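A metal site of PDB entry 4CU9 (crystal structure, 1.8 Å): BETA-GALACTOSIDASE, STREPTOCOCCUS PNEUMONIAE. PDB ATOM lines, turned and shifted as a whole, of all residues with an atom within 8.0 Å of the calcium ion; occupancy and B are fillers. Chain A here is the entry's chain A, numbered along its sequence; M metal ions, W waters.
The backbone NH of Gly 41 is in hydrogen-bond range of the side-chain carboxylate of Glu 178 (2.9 Å). O of Glu 178 lies within hydrogen-bond range of N of His 85 (2.9 Å). The backbone NH (N) of Ile 177 sits at hydrogen-bond distance from the backbone carbonyl oxygen (O) of His 85, at 2.7 Å. The side-chain carboxylate of Asp 42 is in salt-bridge range of the guanidinium group of Arg 47 (3.5 Å). The side-chain carboxylate (OD1) of Asp 42 is in hydrogen-bond range of the side-chain hydroxyl (OG) of Ser 44 (2.6 Å). The guanidinium group of Arg 47 is in salt-bridge range of the side-chain carboxylate of Asp 40 (2.8 Å).
Within 4 Å of the calcium ion: Tyr 37, Asp 40, Asp 42, Ile 177 and Glu 178. Along chain A the residues within 4 Å of the calcium ion span positions 37 to 178.
The calcium ion is bound by OE1 of Glu 178. O of Tyr 37 is bound to the calcium ion (2.2 Å). The calcium ion is bound by the backbone carbonyl oxygen (O) of Ile 177. Water W1 is bound to the calcium ion. The calcium ion is bound by O of Asp 42 (2.4 Å). The calcium ion is bound by OD1 of Asp 40 (2.4 Å).
Water W1 lies within hydrogen-bond range of the backbone carbonyl oxygen of Arg 47 (2.6 Å) and the side-chain carboxylate of Asp 42 (2.8 Å).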
ATOM      1  N   ARG A  34      11.481   9.909  34.881  1.00  0.00           N
ATOM      2  CA  ARG A  34      10.132   9.610  35.340  1.00  0.00           C
ATOM      3  C   ARG A  34       9.681   8.299  34.723  1.00  0.00           C
ATOM      4  O   ARG A  34       9.889   8.061  33.520  1.00  0.00           O
ATOM      5  CB  ARG A  34       9.133  10.708  34.900  1.00  0.00           C
ATOM      6  CG  ARG A  34       9.393  12.126  35.410  1.00  0.00           C
ATOM      7  CD  ARG A  34       9.281  12.214  36.934  1.00  0.00           C
ATOM      8  NE  ARG A  34       9.550  13.594  37.434  1.00  0.00           N
ATOM      9  CZ  ARG A  34      10.717  14.048  37.886  1.00  0.00           C
ATOM     10  NH1 ARG A  34      11.814  13.272  37.991  1.00  0.00           N
ATOM     11  NH2 ARG A  34      10.788  15.314  38.299  1.00  0.00           N
ATOM     12  N   VAL A  35       9.053   7.463  35.522  1.00  0.00           N
ATOM     13  CA  VAL A  35       8.561   6.173  35.019  1.00  0.00           C
ATOM     14  C   VAL A  35       7.396   6.400  34.031  1.00  0.00           C
ATOM     15  O   VAL A  35       7.173   5.614  33.123  1.00  0.00           O
ATOM     16  CB  VAL A  35       8.129   5.258  36.150  1.00  0.00           C
ATOM     17  CG1 VAL A  35       6.799   5.709  36.764  1.00  0.00           C
ATOM     18  CG2 VAL A  35       8.017   3.832  35.665  1.00  0.00           C
ATOM     19  N   ASP A  36       6.664   7.483  34.207  1.00  0.00           N
ATOM     20  CA  ASP A  36       5.564   7.782  33.318  1.00  0.00           C
ATOM     21  C   ASP A  36       6.029   8.076  31.907  1.00  0.00           C
ATOM     22  O   ASP A  36       5.239   8.033  30.991  1.00  0.00           O
ATOM     23  CB  ASP A  36       4.731   8.947  33.888  1.00  0.00           C
ATOM     24  CG  ASP A  36       3.834   8.497  35.061  1.00  0.00           C
ATOM     25  OD1 ASP A  36       3.054   7.519  34.915  1.00  0.00           O
ATOM     26  OD2 ASP A  36       3.882   9.114  36.150  1.00  0.00           O
ATOM     27  N   TYR A  37       7.320   8.344  31.693  1.00  0.00           N
ATOM     28  CA  TYR A  37       7.840   8.524  30.352  1.00  0.00           C
ATOM     29  C   TYR A  37       7.937   7.201  29.573  1.00  0.00           C
ATOM     30  O   TYR A  37       8.113   7.231  28.357  1.00  0.00           O
ATOM     31  CB  TYR A  37       9.218   9.184  30.359  1.00  0.00           C
ATOM     32  CG  TYR A  37       9.248  10.595  30.882  1.00  0.00           C
ATOM     33  CD1 TYR A  37       8.152  11.429  30.749  1.00  0.00           C
ATOM     34  CD2 TYR A  37      10.382  11.109  31.508  1.00  0.00           C
ATOM     35  CE1 TYR A  37       8.154  12.732  31.235  1.00  0.00           C
ATOM     36  CE2 TYR A  37      10.406  12.439  31.964  1.00  0.00           C
ATOM     37  CZ  TYR A  37       9.282  13.240  31.825  1.00  0.00           C
ATOM     38  OH  TYR A  37       9.223  14.555  32.294  1.00  0.00           O
ATOM     39  N   LEU A  38       7.776   6.064  30.266  1.00  0.00           N
ATOM     40  CA  LEU A  38       7.802   4.756  29.631  1.00  0.00           C
ATOM     41  C   LEU A  38       6.653   4.492  28.656  1.00  0.00           C
ATOM     42  O   LEU A  38       6.841   3.748  27.700  1.00  0.00           O
ATOM     43  CB  LEU A  38       7.753   3.635  30.649  1.00  0.00           C
ATOM     44  CG  LEU A  38       9.004   3.324  31.455  1.00  0.00           C
ATOM     45  CD1 LEU A  38       8.716   2.129  32.339  1.00  0.00           C
ATOM     46  CD2 LEU A  38      10.165   3.002  30.549  1.00  0.00           C
ATOM     47  N   ASN A  39       5.480   5.052  28.926  1.00  0.00           N
ATOM     48  CA  ASN A  39       4.341   4.809  28.028  1.00  0.00           C
ATOM     49  C   ASN A  39       3.613   6.037  27.558  1.00  0.00           C
ATOM     50  O   ASN A  39       2.397   6.012  27.410  1.00  0.00           O
ATOM     51  CB  ASN A  39       3.349   3.819  28.671  1.00  0.00           C
ATOM     52  CG  ASN A  39       2.667   4.386  29.896  1.00  0.00           C
ATOM     53  OD1 ASN A  39       3.191   5.277  30.526  1.00  0.00           O
ATOM     54  ND2 ASN A  39       1.485   3.855  30.225  1.00  0.00           N
ATOM     55  N   ASP A  40       4.353   7.092  27.265  1.00  0.00           N
ATOM     56  CA  ASP A  40       3.732   8.347  26.834  1.00  0.00           C
ATOM     57  C   ASP A  40       3.743   8.513  25.313  1.00  0.00           C
ATOM     58  O   ASP A  40       3.375   9.550  24.789  1.00  0.00           O
ATOM     59  CB  ASP A  40       4.414   9.542  27.514  1.00  0.00           C
ATOM     60  CG  ASP A  40       5.854   9.695  27.127  1.00  0.00           C
ATOM     61  OD1 ASP A  40       6.436   8.888  26.373  1.00  0.00           O
ATOM     62  OD2 ASP A  40       6.441  10.651  27.586  1.00  0.00           O
ATOM     63  N   GLY A  41       4.187   7.492  24.582  1.00  0.00           N
ATOM     64  CA  GLY A  41       4.275   7.612  23.131  1.00  0.00           C
ATOM     65  C   GLY A  41       5.446   8.419  22.611  1.00  0.00           C
ATOM     66  O   GLY A  41       5.692   8.407  21.407  1.00  0.00           O
ATOM     67  N   ASP A  42       6.152   9.115  23.512  1.00  0.00           N
ATOM     68  CA  ASP A  42       7.223  10.021  23.138  1.00  0.00           C
ATOM     69  C   ASP A  42       8.539   9.238  23.115  1.00  0.00           C
ATOM     70  O   ASP A  42       8.773   8.393  23.960  1.00  0.00           O
ATOM     71  CB  ASP A  42       7.286  11.209  24.123  1.00  0.00           C
ATOM     72  CG  ASP A  42       8.576  11.979  24.018  1.00  0.00           C
ATOM     73  OD1 ASP A  42       8.652  12.906  23.185  1.00  0.00           O
ATOM     74  OD2 ASP A  42       9.560  11.622  24.720  1.00  0.00           O
ATOM     75  N   HIS A  43       9.375   9.540  22.129  1.00  0.00           N
ATOM     76  CA  HIS A  43      10.672   8.890  22.007  1.00  0.00           C
ATOM     77  C   HIS A  43      11.828   9.874  22.103  1.00  0.00           C
ATOM     78  O   HIS A  43      12.883   9.621  21.575  1.00  0.00           O
ATOM     79  CB  HIS A  43      10.725   8.038  20.731  1.00  0.00           C
ATOM     80  CG  HIS A  43       9.792   6.862  20.764  1.00  0.00           C
ATOM     81  ND1 HIS A  43      10.190   5.576  21.093  1.00  0.00           N
ATOM     82  CD2 HIS A  43       8.457   6.784  20.537  1.00  0.00           C
ATOM     83  CE1 HIS A  43       9.150   4.772  21.065  1.00  0.00           C
ATOM     84  NE2 HIS A  43       8.082   5.474  20.721  1.00  0.00           N
ATOM     85  N   SER A  44      11.644  10.975  22.840  1.00  0.00           N
ATOM     86  CA  SER A  44      12.713  11.925  23.084  1.00  0.00           C
ATOM     87  C   SER A  44      13.722  11.328  24.069  1.00  0.00           C
ATOM     88  O   SER A  44      13.333  10.818  25.127  1.00  0.00           O
ATOM     89  CB  SER A  44      12.162  13.225  23.691  1.00  0.00           C
ATOM     90  OG  SER A  44      11.057  13.731  22.952  1.00  0.00           O
ATOM     91  N   GLU A  45      15.007  11.455  23.752  1.00  0.00           N
ATOM     92  CA  GLU A  45      16.086  11.003  24.632  1.00  0.00           C
ATOM     93  C   GLU A  45      16.102  11.706  25.981  1.00  0.00           C
ATOM     94  O   GLU A  45      16.617  11.157  26.967  1.00  0.00           O
ATOM     95  CB  GLU A  45      17.455  11.149  23.934  1.00  0.00           C
ATOM     96  CG  GLU A  45      17.516  10.342  22.658  1.00  0.00           C
ATOM     97  CD  GLU A  45      18.904  10.213  22.055  1.00  0.00           C
ATOM     98  OE1 GLU A  45      19.866  10.837  22.548  1.00  0.00           O
ATOM     99  OE2 GLU A  45      19.013   9.468  21.062  1.00  0.00           O
ATOM    100  N   ARG A  47      13.423  12.478  27.770  1.00  0.00           N
ATOM    101  CA  ARG A  47      12.333  12.013  28.597  1.00  0.00           C
ATOM    102  C   ARG A  47      12.481  10.512  28.808  1.00  0.00           C
ATOM    103  O   ARG A  47      11.938   9.712  28.049  1.00  0.00           O
ATOM    104  CB  ARG A  47      10.996  12.332  27.968  1.00  0.00           C
ATOM    105  CG  ARG A  47      10.683  13.821  27.864  1.00  0.00           C
ATOM    106  CD  ARG A  47       9.474  14.088  26.974  1.00  0.00           C
ATOM    107  NE  ARG A  47       8.243  13.399  27.440  1.00  0.00           N
ATOM    108  CZ  ARG A  47       7.354  13.933  28.283  1.00  0.00           C
ATOM    109  NH1 ARG A  47       7.531  15.153  28.796  1.00  0.00           N
ATOM    110  NH2 ARG A  47       6.260  13.257  28.635  1.00  0.00           N
ATOM    111  N   ARG A  48      13.224  10.130  29.819  1.00  0.00           N
ATOM    112  CA  ARG A  48      13.485   8.710  30.049  1.00  0.00           C
ATOM    113  C   ARG A  48      13.181   8.299  31.482  1.00  0.00           C
ATOM    114  O   ARG A  48      13.100   9.133  32.388  1.00  0.00           O
ATOM    115  CB  ARG A  48      14.930   8.395  29.715  1.00  0.00           C
ATOM    116  CG  ARG A  48      15.899   9.193  30.552  1.00  0.00           C
ATOM    117  CD  ARG A  48      17.197   9.400  29.850  1.00  0.00           C
ATOM    118  NE  ARG A  48      18.090  10.161  30.724  1.00  0.00           N
ATOM    119  CZ  ARG A  48      18.601  11.359  30.454  1.00  0.00           C
ATOM    120  NH1 ARG A  48      18.348  11.983  29.319  1.00  0.00           N
ATOM    121  NH2 ARG A  48      19.393  11.934  31.324  1.00  0.00           N
ATOM    122  N   TRP A  49      12.919   7.019  31.653  1.00  0.00           N
ATOM    123  CA  TRP A  49      12.947   6.390  32.939  1.00  0.00           C
ATOM    124  C   TRP A  49      14.342   5.822  33.139  1.00  0.00           C
ATOM    125  O   TRP A  49      14.937   5.235  32.246  1.00  0.00           O
ATOM    126  CB  TRP A  49      11.900   5.268  33.020  1.00  0.00           C
ATOM    127  CG  TRP A  49      12.137   4.415  34.216  1.00  0.00           C
ATOM    128  CD1 TRP A  49      11.724   4.666  35.488  1.00  0.00           C
ATOM    129  CD2 TRP A  49      12.873   3.219  34.260  1.00  0.00           C
ATOM    130  NE1 TRP A  49      12.140   3.667  36.325  1.00  0.00           N
ATOM    131  CE2 TRP A  49      12.863   2.765  35.591  1.00  0.00           C
ATOM    132  CE3 TRP A  49      13.530   2.443  33.290  1.00  0.00           C
ATOM    133  CZ2 TRP A  49      13.493   1.595  35.986  1.00  0.00           C
ATOM    134  CZ3 TRP A  49      14.148   1.297  33.677  1.00  0.00           C
ATOM    135  CH2 TRP A  49      14.150   0.885  35.016  1.00  0.00           C
ATOM    136  N   HIS A  85      12.523   0.551  23.963  1.00  0.00           N
ATOM    137  CA  HIS A  85      13.463   1.594  23.503  1.00  0.00           C
ATOM    138  C   HIS A  85      14.388   1.961  24.659  1.00  0.00           C
ATOM    139  O   HIS A  85      13.944   2.622  25.617  1.00  0.00           O
ATOM    140  CB  HIS A  85      12.699   2.829  23.060  1.00  0.00           C
ATOM    141  CG  HIS A  85      13.475   3.797  22.224  1.00  0.00           C
ATOM    142  ND1 HIS A  85      14.840   3.720  22.052  1.00  0.00           N
ATOM    143  CD2 HIS A  85      13.061   4.865  21.502  1.00  0.00           C
ATOM    144  CE1 HIS A  85      15.231   4.702  21.243  1.00  0.00           C
ATOM    145  NE2 HIS A  85      14.172   5.398  20.890  1.00  0.00           N
ATOM    146  N   MET A 176      15.423   3.709  29.874  1.00  0.00           N
ATOM    147  CA  MET A 176      14.460   3.435  28.819  1.00  0.00           C
ATOM    148  C   MET A 176      13.664   4.642  28.451  1.00  0.00           C
ATOM    149  O   MET A 176      13.272   5.459  29.320  1.00  0.00           O
ATOM    150  CB  MET A 176      13.438   2.323  29.193  1.00  0.00           C
ATOM    151  CG  MET A 176      14.017   1.011  29.618  1.00  0.00           C
ATOM    152  SD  MET A 176      12.782  -0.297  29.844  1.00  0.00           S
ATOM    153  CE  MET A 176      12.300  -0.646  28.176  1.00  0.00           C
ATOM    154  N   ILE A 177      13.364   4.724  27.160  1.00  0.00           N
ATOM    155  CA  ILE A 177      12.565   5.803  26.615  1.00  0.00           C
ATOM    156  C   ILE A 177      11.111   5.391  26.388  1.00  0.00           C
ATOM    157  O   ILE A 177      10.227   6.231  26.431  1.00  0.00           O
ATOM    158  CB  ILE A 177      13.217   6.310  25.313  1.00  0.00           C
ATOM    159  CG1 ILE A 177      14.505   7.044  25.666  1.00  0.00           C
ATOM    160  CG2 ILE A 177      12.295   7.216  24.517  1.00  0.00           C
ATOM    161  CD1 ILE A 177      15.467   7.121  24.479  1.00  0.00           C
ATOM    162  N   GLU A 178      10.893   4.119  26.074  1.00  0.00           N
ATOM    163  CA  GLU A 178       9.559   3.625  25.860  1.00  0.00           C
ATOM    164  C   GLU A 178       9.497   2.122  26.099  1.00  0.00           C
ATOM    165  O   GLU A 178      10.437   1.382  25.829  1.00  0.00           O
ATOM    166  CB  GLU A 178       9.040   3.989  24.461  1.00  0.00           C
ATOM    167  CG  GLU A 178       7.532   3.846  24.288  1.00  0.00           C
ATOM    168  CD  GLU A 178       6.705   4.966  24.886  1.00  0.00           C
ATOM    169  OE1 GLU A 178       7.281   5.973  25.399  1.00  0.00           O
ATOM    170  OE2 GLU A 178       5.454   4.875  24.825  1.00  0.00           O
ATOM    171  N   MET A 179       8.348   1.701  26.628  1.00  0.00           N
ATOM    172  CA  MET A 179       8.069   0.282  26.807  1.00  0.00           C
ATOM    173  C   MET A 179       6.603   0.115  26.455  1.00  0.00           C
ATOM    174  O   MET A 179       5.764   0.810  27.035  1.00  0.00           O
ATOM    175  CB  MET A 179       8.315  -0.121  28.250  1.00  0.00           C
ATOM    176  CG  MET A 179       7.847  -1.501  28.611  1.00  0.00           C
ATOM    177  SD  MET A 179       8.077  -1.901  30.334  1.00  0.00           S
ATOM    178  CE  MET A 179       9.812  -1.754  30.620  1.00  0.00           C
ATOM    179  N   THR A 180       6.294  -0.809  25.563  1.00  0.00           N
ATOM    180  CA  THR A 180       4.933  -1.036  25.079  1.00  0.00           C
ATOM    181  C   THR A 180       4.649  -2.536  25.000  1.00  0.00           C
ATOM    182  O   THR A 180       5.562  -3.344  24.657  1.00  0.00           O
ATOM    183  CB  THR A 180       4.753  -0.433  23.670  1.00  0.00           C
ATOM    184  OG1 THR A 180       5.352   0.867  23.607  1.00  0.00           O
ATOM    185  CG2 THR A 180       3.316  -0.268  23.327  1.00  0.00           C
HETATM  186 CA    CA M   1       8.470   7.688  26.193  1.00  0.00          CA
HETATM  187  O   HOH W   1       9.857   9.517  26.502  1.00  0.00           O
